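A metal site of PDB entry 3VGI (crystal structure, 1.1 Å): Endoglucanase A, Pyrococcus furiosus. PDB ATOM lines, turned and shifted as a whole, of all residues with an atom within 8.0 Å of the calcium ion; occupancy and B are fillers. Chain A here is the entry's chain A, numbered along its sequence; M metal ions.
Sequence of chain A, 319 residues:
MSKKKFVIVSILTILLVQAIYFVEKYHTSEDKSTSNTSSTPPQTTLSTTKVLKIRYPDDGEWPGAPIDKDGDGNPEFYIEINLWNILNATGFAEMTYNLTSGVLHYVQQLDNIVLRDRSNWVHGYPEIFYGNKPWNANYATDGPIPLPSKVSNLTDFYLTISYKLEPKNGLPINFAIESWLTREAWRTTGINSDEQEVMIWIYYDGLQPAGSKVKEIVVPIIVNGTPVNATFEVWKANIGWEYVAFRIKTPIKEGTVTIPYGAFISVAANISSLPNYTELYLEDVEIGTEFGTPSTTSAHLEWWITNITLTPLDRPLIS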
ATOM      1  N   ILE A  67     -12.119   0.439 -14.822  1.00  0.00           N
ATOM      2  CA  ILE A  67     -10.881   0.412 -14.018  1.00  0.00           C
ATOM      3  C   ILE A  67     -10.400  -1.043 -14.074  1.00  0.00           C
ATOM      4  O   ILE A  67     -11.107  -1.946 -13.635  1.00  0.00           O
ATOM      5  CB  ILE A  67     -11.155   0.826 -12.603  1.00  0.00           C
ATOM      6  CG1 ILE A  67     -11.525   2.381 -12.629  1.00  0.00           C
ATOM      7  CG2 ILE A  67      -9.925   0.527 -11.727  1.00  0.00           C
ATOM      8  CD1 ILE A  67     -11.995   2.894 -11.283  1.00  0.00           C
ATOM      9  N   ASP A  68      -9.228  -1.211 -14.702  1.00  0.00           N
ATOM     10  CA  ASP A  68      -8.752  -2.579 -14.954  1.00  0.00           C
ATOM     11  C   ASP A  68      -7.234  -2.520 -14.679  1.00  0.00           C
ATOM     12  O   ASP A  68      -6.403  -2.458 -15.570  1.00  0.00           O
ATOM     13  CB  ASP A  68      -9.026  -2.967 -16.420  1.00  0.00           C
ATOM     14  CG  ASP A  68      -8.619  -4.388 -16.730  1.00  0.00           C
ATOM     15  OD1 ASP A  68      -8.263  -5.185 -15.814  1.00  0.00           O
ATOM     16  OD2 ASP A  68      -8.552  -4.694 -17.960  1.00  0.00           O
ATOM     17  N   LYS A  69      -6.884  -2.571 -13.390  1.00  0.00           N
ATOM     18  CA  LYS A  69      -5.531  -2.262 -12.995  1.00  0.00           C
ATOM     19  C   LYS A  69      -4.520  -3.272 -13.491  1.00  0.00           C
ATOM     20  O   LYS A  69      -3.365  -2.922 -13.720  1.00  0.00           O
ATOM     21  CB  LYS A  69      -5.406  -2.136 -11.491  1.00  0.00           C
ATOM     22  CG  LYS A  69      -3.995  -1.857 -11.038  1.00  0.00           C
ATOM     23  CD  LYS A  69      -4.047  -1.403  -9.601  1.00  0.00           C
ATOM     24  CE  LYS A  69      -2.664  -1.474  -8.990  1.00  0.00           C
ATOM     25  NZ  LYS A  69      -1.740  -0.502  -9.615  1.00  0.00           N
ATOM     26  N   ASP A  70      -4.913  -4.533 -13.619  1.00  0.00           N
ATOM     27  CA  ASP A  70      -4.032  -5.582 -14.083  1.00  0.00           C
ATOM     28  C   ASP A  70      -4.129  -5.759 -15.606  1.00  0.00           C
ATOM     29  O   ASP A  70      -3.403  -6.576 -16.180  1.00  0.00           O
ATOM     30  CB  ASP A  70      -4.252  -6.913 -13.305  1.00  0.00           C
ATOM     31  CG  ASP A  70      -5.601  -7.527 -13.474  1.00  0.00           C
ATOM     32  OD1 ASP A  70      -6.567  -6.852 -13.913  1.00  0.00           O
ATOM     33  OD2 ASP A  70      -5.802  -8.728 -13.131  1.00  0.00           O
ATOM     34  N   GLY A  71      -4.938  -4.914 -16.277  1.00  0.00           N
ATOM     35  CA  GLY A  71      -5.021  -4.950 -17.748  1.00  0.00           C
ATOM     36  C   GLY A  71      -5.487  -6.336 -18.252  1.00  0.00           C
ATOM     37  O   GLY A  71      -5.108  -6.719 -19.367  1.00  0.00           O
ATOM     38  N   ASP A  72      -6.295  -7.054 -17.537  1.00  0.00           N
ATOM     39  CA  ASP A  72      -6.664  -8.396 -17.932  1.00  0.00           C
ATOM     40  C   ASP A  72      -7.990  -8.419 -18.678  1.00  0.00           C
ATOM     41  O   ASP A  72      -8.500  -9.533 -19.033  1.00  0.00           O
ATOM     42  CB  ASP A  72      -6.627  -9.360 -16.752  1.00  0.00           C
ATOM     43  CG  ASP A  72      -7.858  -9.323 -15.862  1.00  0.00           C
ATOM     44  OD1 ASP A  72      -8.615  -8.308 -15.867  1.00  0.00           O
ATOM     45  OD2 ASP A  72      -8.056 -10.315 -15.055  1.00  0.00           O
ATOM     46  N   GLY A  73      -8.612  -7.289 -18.958  1.00  0.00           N
ATOM     47  CA  GLY A  73      -9.852  -7.277 -19.745  1.00  0.00           C
ATOM     48  C   GLY A  73     -11.097  -7.513 -18.945  1.00  0.00           C
ATOM     49  O   GLY A  73     -12.206  -7.521 -19.526  1.00  0.00           O
ATOM     50  N   ASN A  74     -11.006  -7.671 -17.604  1.00  0.00           N
ATOM     51  CA  ASN A  74     -12.134  -7.806 -16.726  1.00  0.00           C
ATOM     52  C   ASN A  74     -12.020  -6.661 -15.700  1.00  0.00           C
ATOM     53  O   ASN A  74     -11.106  -6.688 -14.869  1.00  0.00           O
ATOM     54  CB  ASN A  74     -12.128  -9.162 -16.004  1.00  0.00           C
ATOM     55  CG  ASN A  74     -13.425  -9.425 -15.290  1.00  0.00           C
ATOM     56  OD1 ASN A  74     -14.379  -8.610 -15.365  1.00  0.00           O
ATOM     57  ND2 ASN A  74     -13.447 -10.540 -14.532  1.00  0.00           N
ATOM     58  N   PRO A  75     -12.838  -5.638 -15.798  1.00  0.00           N
ATOM     59  CA  PRO A  75     -12.613  -4.473 -14.886  1.00  0.00           C
ATOM     60  C   PRO A  75     -12.910  -4.923 -13.436  1.00  0.00           C
ATOM     61  O   PRO A  75     -13.825  -5.717 -13.165  1.00  0.00           O
ATOM     62  CB  PRO A  75     -13.663  -3.447 -15.389  1.00  0.00           C
ATOM     63  CG  PRO A  75     -13.924  -3.884 -16.819  1.00  0.00           C
ATOM     64  CD  PRO A  75     -13.889  -5.397 -16.765  1.00  0.00           C
ATOM     65  N   GLU A  76     -12.154  -4.283 -12.509  1.00  0.00           N
ATOM     66  CA  GLU A  76     -12.496  -4.373 -11.092  1.00  0.00           C
ATOM     67  C   GLU A  76     -13.685  -3.494 -10.684  1.00  0.00           C
ATOM     68  O   GLU A  76     -14.458  -3.833  -9.791  1.00  0.00           O
ATOM     69  CB  GLU A  76     -11.282  -3.991 -10.213  1.00  0.00           C
ATOM     70  CG  GLU A  76     -10.072  -4.887 -10.457  1.00  0.00           C
ATOM     71  CD  GLU A  76      -9.199  -4.363 -11.612  1.00  0.00           C
ATOM     72  OE1 GLU A  76      -8.834  -3.189 -11.507  1.00  0.00           O
ATOM     73  OE2 GLU A  76      -8.864  -5.077 -12.575  1.00  0.00           O
ATOM     74  N   PHE A  77     -13.766  -2.346 -11.400  1.00  0.00           N
ATOM     75  CA  PHE A  77     -14.888  -1.414 -11.155  1.00  0.00           C
ATOM     76  C   PHE A  77     -15.090  -0.693 -12.508  1.00  0.00           C
ATOM     77  O   PHE A  77     -14.235  -0.778 -13.404  1.00  0.00           O
ATOM     78  CB  PHE A  77     -14.546  -0.329 -10.101  1.00  0.00           C
ATOM     79  CG  PHE A  77     -14.380  -0.913  -8.717  1.00  0.00           C
ATOM     80  CD1 PHE A  77     -15.515  -1.195  -7.945  1.00  0.00           C
ATOM     81  CD2 PHE A  77     -13.115  -1.238  -8.211  1.00  0.00           C
ATOM     82  CE1 PHE A  77     -15.354  -1.816  -6.682  1.00  0.00           C
ATOM     83  CE2 PHE A  77     -12.991  -1.825  -6.969  1.00  0.00           C
ATOM     84  CZ  PHE A  77     -14.106  -2.138  -6.193  1.00  0.00           C
ATOM     85  N   THR A 141     -16.359  -7.314 -13.261  1.00  0.00           N
ATOM     86  CA  THR A 141     -16.575  -8.564 -12.512  1.00  0.00           C
ATOM     87  C   THR A 141     -15.293  -9.140 -11.942  1.00  0.00           C
ATOM     88  O   THR A 141     -15.291 -10.307 -11.468  1.00  0.00           O
ATOM     89  CB  THR A 141     -17.334  -9.635 -13.373  1.00  0.00           C
ATOM     90  OG1 THR A 141     -16.548 -10.035 -14.471  1.00  0.00           O
ATOM     91  CG2 THR A 141     -18.709  -9.097 -13.751  1.00  0.00           C
ATOM     92  N   ASP A 142     -14.249  -8.345 -11.852  1.00  0.00           N
ATOM     93  CA  ASP A 142     -12.952  -8.794 -11.303  1.00  0.00           C
ATOM     94  C   ASP A 142     -13.001  -8.485  -9.798  1.00  0.00           C
ATOM     95  O   ASP A 142     -12.529  -7.410  -9.386  1.00  0.00           O
ATOM     96  CB  ASP A 142     -11.824  -8.165 -12.066  1.00  0.00           C
ATOM     97  CG  ASP A 142     -10.464  -8.735 -11.726  1.00  0.00           C
ATOM     98  OD1 ASP A 142     -10.324  -9.535 -10.784  1.00  0.00           O
ATOM     99  OD2 ASP A 142      -9.490  -8.318 -12.461  1.00  0.00           O
ATOM    100  N   GLY A 143     -13.570  -9.341  -8.974  1.00  0.00           N
ATOM    101  CA  GLY A 143     -13.711  -9.091  -7.535  1.00  0.00           C
ATOM    102  C   GLY A 143     -14.187 -10.383  -6.863  1.00  0.00           C
ATOM    103  O   GLY A 143     -14.522 -11.365  -7.527  1.00  0.00           O
HETATM  104 CA    CA M   1      -8.879  -6.742 -14.119  1.00  0.00          CA
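The side-chain carboxylate (OE1) of Glu 76 lies within hydrogen-bond range of the backbone NH (N) of Lys 69 (2.8 Å). The backbone carbonyl oxygen (O) of Ile 67 is in hydrogen-bond range of the backbone NH (N) of Glu 76, at 2.8 Å. The side-chain amide oxygen of Asn 74 lies within hydrogen-bond range of the side-chain hydroxyl of Thr 141, at 2.7 Å. O of Pro 75 is in hydrogen-bond range of N of Asp 142 (3.0 Å). The backbone NH of Gly 71 lies close to the side-chain carboxylate of Asp 68, at 3.4 Å. The backbone NH (N) of Gly 73 is in hydrogen-bond range of the side-chain carboxylate (OD2) of Asp 68 (2.8 Å).
The nearest printed residue that does not touch the calcium ion is Pro 75 (4.4 Å).
The calcium ion is bound by OE2 of Glu 76 (2.3 Å), OD1 of Asp 70 (2.3 Å), O of Asn 74 (2.4 Å), OD1 of Asp 72 (2.4 Å), OD2 of Asp 142 (2.4 Å) and OD1 of Asp 68 (2.4 Å). The calcium ion has six donor atoms within binding distance.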
